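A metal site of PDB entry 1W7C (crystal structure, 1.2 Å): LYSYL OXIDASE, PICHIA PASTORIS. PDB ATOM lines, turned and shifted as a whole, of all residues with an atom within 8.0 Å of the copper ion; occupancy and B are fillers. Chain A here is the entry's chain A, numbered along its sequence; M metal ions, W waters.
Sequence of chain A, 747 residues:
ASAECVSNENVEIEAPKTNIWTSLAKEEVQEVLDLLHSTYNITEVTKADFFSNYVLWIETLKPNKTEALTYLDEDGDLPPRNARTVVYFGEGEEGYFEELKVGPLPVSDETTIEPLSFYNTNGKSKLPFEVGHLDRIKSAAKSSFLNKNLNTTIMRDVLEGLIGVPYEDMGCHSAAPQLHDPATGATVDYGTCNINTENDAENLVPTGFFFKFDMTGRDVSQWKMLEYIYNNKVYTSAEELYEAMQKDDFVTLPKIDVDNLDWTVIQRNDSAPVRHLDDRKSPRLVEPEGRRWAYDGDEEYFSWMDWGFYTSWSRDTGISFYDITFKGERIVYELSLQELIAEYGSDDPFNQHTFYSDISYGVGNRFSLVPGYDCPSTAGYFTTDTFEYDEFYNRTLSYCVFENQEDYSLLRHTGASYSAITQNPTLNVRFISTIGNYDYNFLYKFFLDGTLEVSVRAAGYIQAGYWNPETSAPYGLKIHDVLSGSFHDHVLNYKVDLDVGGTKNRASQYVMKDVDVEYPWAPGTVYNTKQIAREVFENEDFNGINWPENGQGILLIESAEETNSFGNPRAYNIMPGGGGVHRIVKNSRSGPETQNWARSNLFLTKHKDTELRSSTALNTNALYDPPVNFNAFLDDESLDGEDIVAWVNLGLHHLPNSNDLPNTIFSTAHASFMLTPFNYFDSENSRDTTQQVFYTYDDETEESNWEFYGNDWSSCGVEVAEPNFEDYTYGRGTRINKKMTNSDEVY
OH of Tyr 440 is in hydrogen-bond range of ND1 of His 490 (3.2 Å).
NE2 of His 654 is in hydrogen-bond range of OD1 of Asp 660.
A ring nitrogen (ND1) of His 488 lies within hydrogen-bond range of the backbone carbonyl oxygen (O) of Ser 486 (3.0 Å).
The backbone NH of Leu 652 is in hydrogen-bond range of the backbone carbonyl oxygen of His 490, at 2.9 Å.
Three residues have an atom within 4 Å of the copper ion: His 488, His 490 and His 654.
The nearest printed residue that does not touch the copper ion is Ile 462 (5.2 Å).
The copper ion is bound by ND1 of His 654 (2.0 Å), NE2 of His 488 (2.0 Å), NE2 of His 490 (2.0 Å) and water W1 (2.2 Å).
The copper ion has four donor atoms within binding distance.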
ATOM      1  N   ALA A 342      18.055 -15.164  25.936  1.00  0.00           N
ATOM      2  CA  ALA A 342      19.055 -14.190  25.573  1.00  0.00           C
ATOM      3  C   ALA A 342      19.373 -14.412  24.114  1.00  0.00           C
ATOM      4  O   ALA A 342      19.982 -15.445  23.759  1.00  0.00           O
ATOM      5  CB  ALA A 342      20.301 -14.306  26.429  1.00  0.00           C
ATOM      6  N   TYR A 344      20.939 -13.033  20.582  1.00  0.00           N
ATOM      7  CA  TYR A 344      22.000 -12.141  20.081  1.00  0.00           C
ATOM      8  C   TYR A 344      21.847 -11.855  18.611  1.00  0.00           C
ATOM      9  O   TYR A 344      21.393 -12.721  17.860  1.00  0.00           O
ATOM     10  CB  TYR A 344      23.394 -12.740  20.376  1.00  0.00           C
ATOM     11  CG  TYR A 344      23.723 -12.731  21.843  1.00  0.00           C
ATOM     12  CD1 TYR A 344      23.087 -13.596  22.728  1.00  0.00           C
ATOM     13  CD2 TYR A 344      24.663 -11.833  22.393  1.00  0.00           C
ATOM     14  CE1 TYR A 344      23.331 -13.552  24.069  1.00  0.00           C
ATOM     15  CE2 TYR A 344      24.894 -11.791  23.740  1.00  0.00           C
ATOM     16  CZ  TYR A 344      24.220 -12.654  24.564  1.00  0.00           C
ATOM     17  OH  TYR A 344      24.468 -12.588  25.906  1.00  0.00           O
ATOM     18  N   ASN A 437      28.054 -16.751  32.623  1.00  0.00           N
ATOM     19  CA  ASN A 437      28.479 -15.350  32.662  1.00  0.00           C
ATOM     20  C   ASN A 437      27.461 -14.376  33.283  1.00  0.00           C
ATOM     21  O   ASN A 437      27.841 -13.325  33.765  1.00  0.00           O
ATOM     22  CB  ASN A 437      28.838 -14.853  31.243  1.00  0.00           C
ATOM     23  CG  ASN A 437      27.706 -15.041  30.242  1.00  0.00           C
ATOM     24  OD1 ASN A 437      27.261 -16.169  30.017  1.00  0.00           O
ATOM     25  ND2 ASN A 437      27.278 -13.948  29.592  1.00  0.00           N
ATOM     26  N   TPQ A 438      26.168 -14.736  33.227  1.00  0.00           N
ATOM     27  CA  TPQ A 438      25.094 -13.836  33.648  1.00  0.00           C
ATOM     28  CB  TPQ A 438      23.832 -14.026  32.807  1.00  0.00           C
ATOM     29  C   TPQ A 438      24.707 -14.061  35.100  1.00  0.00           C
ATOM     30  O   TPQ A 438      24.636 -15.206  35.545  1.00  0.00           O
ATOM     31  N   TYR A 440      21.489 -13.098  37.390  1.00  0.00           N
ATOM     32  CA  TYR A 440      20.119 -12.583  37.380  1.00  0.00           C
ATOM     33  C   TYR A 440      19.596 -12.497  38.802  1.00  0.00           C
ATOM     34  O   TYR A 440      19.633 -13.460  39.553  1.00  0.00           O
ATOM     35  CB  TYR A 440      19.204 -13.487  36.571  1.00  0.00           C
ATOM     36  CG  TYR A 440      19.544 -13.513  35.119  1.00  0.00           C
ATOM     37  CD1 TYR A 440      19.177 -12.456  34.312  1.00  0.00           C
ATOM     38  CD2 TYR A 440      20.229 -14.580  34.547  1.00  0.00           C
ATOM     39  CE1 TYR A 440      19.479 -12.441  32.942  1.00  0.00           C
ATOM     40  CE2 TYR A 440      20.528 -14.590  33.155  1.00  0.00           C
ATOM     41  CZ  TYR A 440      20.148 -13.509  32.366  1.00  0.00           C
ATOM     42  OH  TYR A 440      20.447 -13.484  31.031  1.00  0.00           O
ATOM     43  N   ALA A 458      19.917  -7.553  35.926  1.00  0.00           N
ATOM     44  CA  ALA A 458      20.979  -8.404  35.395  1.00  0.00           C
ATOM     45  C   ALA A 458      22.372  -7.777  35.658  1.00  0.00           C
ATOM     46  O   ALA A 458      22.557  -6.525  35.662  1.00  0.00           O
ATOM     47  CB  ALA A 458      20.784  -8.619  33.924  1.00  0.00           C
ATOM     48  N   ALA A 459      23.353  -8.608  35.830  1.00  0.00           N
ATOM     49  CA  ALA A 459      24.736  -8.155  35.986  1.00  0.00           C
ATOM     50  C   ALA A 459      25.596  -9.297  35.393  1.00  0.00           C
ATOM     51  O   ALA A 459      25.090 -10.284  34.793  1.00  0.00           O
ATOM     52  CB  ALA A 459      25.111  -7.850  37.490  1.00  0.00           C
ATOM     53  N   GLY A 460      26.870  -9.180  35.588  1.00  0.00           N
ATOM     54  CA  GLY A 460      27.805 -10.215  35.243  1.00  0.00           C
ATOM     55  C   GLY A 460      28.548  -9.819  33.977  1.00  0.00           C
ATOM     56  O   GLY A 460      28.616  -8.638  33.644  1.00  0.00           O
ATOM     57  N   TYR A 461      29.206 -10.812  33.368  1.00  0.00           N
ATOM     58  CA  TYR A 461      29.962 -10.591  32.137  1.00  0.00           C
ATOM     59  C   TYR A 461      29.062 -10.704  30.953  1.00  0.00           C
ATOM     60  O   TYR A 461      28.275 -11.628  30.814  1.00  0.00           O
ATOM     61  CB  TYR A 461      31.053 -11.642  32.010  1.00  0.00           C
ATOM     62  CG  TYR A 461      32.274 -11.440  32.890  1.00  0.00           C
ATOM     63  CD1 TYR A 461      32.509 -12.237  33.996  1.00  0.00           C
ATOM     64  CD2 TYR A 461      33.179 -10.446  32.610  1.00  0.00           C
ATOM     65  CE1 TYR A 461      33.623 -12.025  34.801  1.00  0.00           C
ATOM     66  CE2 TYR A 461      34.299 -10.231  33.391  1.00  0.00           C
ATOM     67  CZ  TYR A 461      34.517 -11.034  34.471  1.00  0.00           C
ATOM     68  OH  TYR A 461      35.624 -10.843  35.266  1.00  0.00           O
ATOM     69  N   ILE A 462      29.237  -9.772  30.040  1.00  0.00           N
ATOM     70  CA  ILE A 462      28.538  -9.869  28.768  1.00  0.00           C
ATOM     71  C   ILE A 462      29.133 -10.953  27.853  1.00  0.00           C
ATOM     72  O   ILE A 462      30.303 -11.262  27.958  1.00  0.00           O
ATOM     73  CB  ILE A 462      28.549  -8.511  28.007  1.00  0.00           C
ATOM     74  CG1 ILE A 462      29.972  -8.087  27.650  1.00  0.00           C
ATOM     75  CG2 ILE A 462      27.835  -7.469  28.793  1.00  0.00           C
ATOM     76  CD1 ILE A 462      30.073  -6.870  26.735  1.00  0.00           C
ATOM     77  N   GLN A 463      28.337 -11.482  26.929  1.00  0.00           N
ATOM     78  CA  GLN A 463      28.843 -12.267  25.837  1.00  0.00           C
ATOM     79  C   GLN A 463      29.160 -11.303  24.708  1.00  0.00           C
ATOM     80  O   GLN A 463      28.313 -10.957  23.917  1.00  0.00           O
ATOM     81  CB  GLN A 463      27.860 -13.354  25.428  1.00  0.00           C
ATOM     82  CG  GLN A 463      28.387 -14.210  24.300  1.00  0.00           C
ATOM     83  CD  GLN A 463      27.497 -15.377  23.935  1.00  0.00           C
ATOM     84  OE1 GLN A 463      27.012 -16.069  24.795  1.00  0.00           O
ATOM     85  NE2 GLN A 463      27.302 -15.603  22.657  1.00  0.00           N
ATOM     86  N   SER A 486      28.334  -7.085  21.745  1.00  0.00           N
ATOM     87  CA  SER A 486      27.281  -7.661  20.930  1.00  0.00           C
ATOM     88  C   SER A 486      25.855  -7.364  21.433  1.00  0.00           C
ATOM     89  O   SER A 486      25.494  -7.598  22.549  1.00  0.00           O
ATOM     90  CB  SER A 486      27.465  -9.176  20.824  1.00  0.00           C
ATOM     91  OG  SER A 486      28.530  -9.507  19.944  1.00  0.00           O
ATOM     92  N   PHE A 487      25.034  -6.935  20.530  1.00  0.00           N
ATOM     93  CA  PHE A 487      23.670  -6.560  20.830  1.00  0.00           C
ATOM     94  C   PHE A 487      22.747  -7.755  21.091  1.00  0.00           C
ATOM     95  O   PHE A 487      22.778  -8.738  20.332  1.00  0.00           O
ATOM     96  CB  PHE A 487      23.249  -5.839  19.565  1.00  0.00           C
ATOM     97  CG  PHE A 487      21.878  -5.242  19.530  1.00  0.00           C
ATOM     98  CD1 PHE A 487      21.245  -5.047  18.287  1.00  0.00           C
ATOM     99  CD2 PHE A 487      21.262  -4.733  20.645  1.00  0.00           C
ATOM    100  CE1 PHE A 487      20.023  -4.439  18.204  1.00  0.00           C
ATOM    101  CE2 PHE A 487      20.005  -4.118  20.534  1.00  0.00           C
ATOM    102  CZ  PHE A 487      19.396  -3.991  19.340  1.00  0.00           C
ATOM    103  N   HIS A 488      21.969  -7.708  22.169  1.00  0.00           N
ATOM    104  CA  HIS A 488      21.102  -8.832  22.489  1.00  0.00           C
ATOM    105  C   HIS A 488      19.872  -8.376  23.238  1.00  0.00           C
ATOM    106  O   HIS A 488      19.853  -7.307  23.848  1.00  0.00           O
ATOM    107  CB  HIS A 488      21.838  -9.916  23.265  1.00  0.00           C
ATOM    108  CG  HIS A 488      22.443  -9.408  24.543  1.00  0.00           C
ATOM    109  ND1 HIS A 488      23.606  -8.657  24.562  1.00  0.00           N
ATOM    110  CD2 HIS A 488      22.046  -9.506  25.847  1.00  0.00           C
ATOM    111  CE1 HIS A 488      23.892  -8.315  25.813  1.00  0.00           C
ATOM    112  NE2 HIS A 488      22.962  -8.820  26.617  1.00  0.00           N
ATOM    113  N   ASP A 489      18.813  -9.189  23.141  1.00  0.00           N
ATOM    114  CA  ASP A 489      17.634  -9.029  23.945  1.00  0.00           C
ATOM    115  C   ASP A 489      17.617 -10.054  25.068  1.00  0.00           C
ATOM    116  O   ASP A 489      17.884 -11.233  24.836  1.00  0.00           O
ATOM    117  CB  ASP A 489      16.368  -9.263  23.112  1.00  0.00           C
ATOM    118  CG  ASP A 489      15.967  -8.078  22.275  1.00  0.00           C
ATOM    119  OD1 ASP A 489      16.419  -6.943  22.563  1.00  0.00           O
ATOM    120  OD2 ASP A 489      15.212  -8.237  21.311  1.00  0.00           O
ATOM    121  N   HIS A 490      17.318  -9.587  26.269  1.00  0.00           N
ATOM    122  CA  HIS A 490      16.889 -10.428  27.387  1.00  0.00           C
ATOM    123  C   HIS A 490      15.367 -10.327  27.426  1.00  0.00           C
ATOM    124  O   HIS A 490      14.843  -9.214  27.420  1.00  0.00           O
ATOM    125  CB  HIS A 490      17.411  -9.891  28.700  1.00  0.00           C
ATOM    126  CG  HIS A 490      18.898  -9.874  28.824  1.00  0.00           C
ATOM    127  ND1 HIS A 490      19.615 -10.943  29.297  1.00  0.00           N
ATOM    128  CD2 HIS A 490      19.789  -8.865  28.636  1.00  0.00           C
ATOM    129  CE1 HIS A 490      20.892 -10.621  29.355  1.00  0.00           C
ATOM    130  NE2 HIS A 490      21.019  -9.359  28.951  1.00  0.00           N
ATOM    131  N   LEU A 652      14.938  -6.420  28.250  1.00  0.00           N
ATOM    132  CA  LEU A 652      15.964  -5.403  28.074  1.00  0.00           C
ATOM    133  C   LEU A 652      16.559  -5.569  26.682  1.00  0.00           C
ATOM    134  O   LEU A 652      16.963  -6.685  26.315  1.00  0.00           O
ATOM    135  CB  LEU A 652      17.099  -5.597  29.087  1.00  0.00           C
ATOM    136  CG  LEU A 652      16.727  -5.651  30.578  1.00  0.00           C
ATOM    137  CD1 LEU A 652      17.854  -6.237  31.444  1.00  0.00           C
ATOM    138  CD2 LEU A 652      16.339  -4.282  31.164  1.00  0.00           C
ATOM    139  N   HIS A 653      16.664  -4.482  25.939  1.00  0.00           N
ATOM    140  CA  HIS A 653      17.491  -4.437  24.752  1.00  0.00           C
ATOM    141  C   HIS A 653      18.881  -3.961  25.177  1.00  0.00           C
ATOM    142  O   HIS A 653      19.068  -2.775  25.477  1.00  0.00           O
ATOM    143  CB  HIS A 653      16.941  -3.455  23.731  1.00  0.00           C
ATOM    144  CG  HIS A 653      15.499  -3.645  23.382  1.00  0.00           C
ATOM    145  ND1 HIS A 653      14.970  -4.875  23.031  1.00  0.00           N
ATOM    146  CD2 HIS A 653      14.469  -2.772  23.385  1.00  0.00           C
ATOM    147  CE1 HIS A 653      13.679  -4.721  22.778  1.00  0.00           C
ATOM    148  NE2 HIS A 653      13.347  -3.458  23.020  1.00  0.00           N
ATOM    149  N   HIS A 654      19.829  -4.866  25.226  1.00  0.00           N
ATOM    150  CA  HIS A 654      21.141  -4.587  25.817  1.00  0.00           C
ATOM    151  C   HIS A 654      22.155  -4.384  24.709  1.00  0.00           C
ATOM    152  O   HIS A 654      22.461  -5.288  23.944  1.00  0.00           O
ATOM    153  CB  HIS A 654      21.551  -5.729  26.719  1.00  0.00           C
ATOM    154  CG  HIS A 654      22.675  -5.416  27.635  1.00  0.00           C
ATOM    155  ND1 HIS A 654      23.200  -6.365  28.485  1.00  0.00           N
ATOM    156  CD2 HIS A 654      23.292  -4.256  27.946  1.00  0.00           C
ATOM    157  CE1 HIS A 654      24.160  -5.813  29.227  1.00  0.00           C
ATOM    158  NE2 HIS A 654      24.233  -4.533  28.910  1.00  0.00           N
ATOM    159  N   LEU A 655      22.685  -3.159  24.660  1.00  0.00           N
ATOM    160  CA  LEU A 655      23.747  -2.731  23.744  1.00  0.00           C
ATOM    161  C   LEU A 655      24.914  -2.316  24.641  1.00  0.00           C
ATOM    162  O   LEU A 655      25.034  -1.134  25.065  1.00  0.00           O
ATOM    163  CB  LEU A 655      23.266  -1.554  22.895  1.00  0.00           C
ATOM    164  CG  LEU A 655      24.290  -1.113  21.845  1.00  0.00           C
ATOM    165  CD1 LEU A 655      24.458  -2.171  20.746  1.00  0.00           C
ATOM    166  CD2 LEU A 655      23.953   0.246  21.234  1.00  0.00           C
ATOM    167  N   PRO A 656      25.760  -3.257  25.030  1.00  0.00           N
ATOM    168  CA  PRO A 656      26.800  -2.962  26.000  1.00  0.00           C
ATOM    169  C   PRO A 656      27.756  -1.852  25.547  1.00  0.00           C
ATOM    170  O   PRO A 656      28.105  -1.738  24.404  1.00  0.00           O
ATOM    171  CB  PRO A 656      27.526  -4.283  26.158  1.00  0.00           C
ATOM    172  CG  PRO A 656      26.437  -5.304  25.905  1.00  0.00           C
ATOM    173  CD  PRO A 656      25.700  -4.710  24.756  1.00  0.00           C
ATOM    174  N   ASP A 660      29.606  -1.428  30.865  1.00  0.00           N
ATOM    175  CA  ASP A 660      29.474  -2.873  31.009  1.00  0.00           C
ATOM    176  C   ASP A 660      30.817  -3.603  31.152  1.00  0.00           C
ATOM    177  O   ASP A 660      30.828  -4.826  31.170  1.00  0.00           O
ATOM    178  CB  ASP A 660      28.692  -3.424  29.830  1.00  0.00           C
ATOM    179  CG  ASP A 660      27.293  -2.899  29.768  1.00  0.00           C
ATOM    180  OD1 ASP A 660      26.431  -3.483  30.473  1.00  0.00           O
ATOM    181  OD2 ASP A 660      27.014  -1.904  29.083  1.00  0.00           O
ATOM    182  N   THR A 664      28.465  -5.729  33.621  1.00  0.00           N
ATOM    183  CA  THR A 664      27.202  -5.024  33.638  1.00  0.00           C
ATOM    184  C   THR A 664      26.787  -4.739  35.076  1.00  0.00           C
ATOM    185  O   THR A 664      27.092  -5.487  35.985  1.00  0.00           O
ATOM    186  CB  THR A 664      26.169  -5.913  32.931  1.00  0.00           C
ATOM    187  OG1 THR A 664      26.549  -6.052  31.551  1.00  0.00           O
ATOM    188  CG2 THR A 664      24.779  -5.318  32.946  1.00  0.00           C
ATOM    189  N   ALA A 669      20.142  -2.077  34.554  1.00  0.00           N
ATOM    190  CA  ALA A 669      19.656  -3.261  33.834  1.00  0.00           C
ATOM    191  C   ALA A 669      18.487  -3.851  34.617  1.00  0.00           C
ATOM    192  O   ALA A 669      18.626  -4.902  35.213  1.00  0.00           O
ATOM    193  CB  ALA A 669      20.789  -4.287  33.670  1.00  0.00           C
HETATM  194 CU    CU M   1      22.708  -8.314  28.558  1.00  0.00          CU
HETATM  195  O   HOH W   1      24.370  -9.528  29.368  1.00  0.00           O
HETATM  196  O   HOH W   2      21.450  -6.524  31.183  1.00  0.00           O
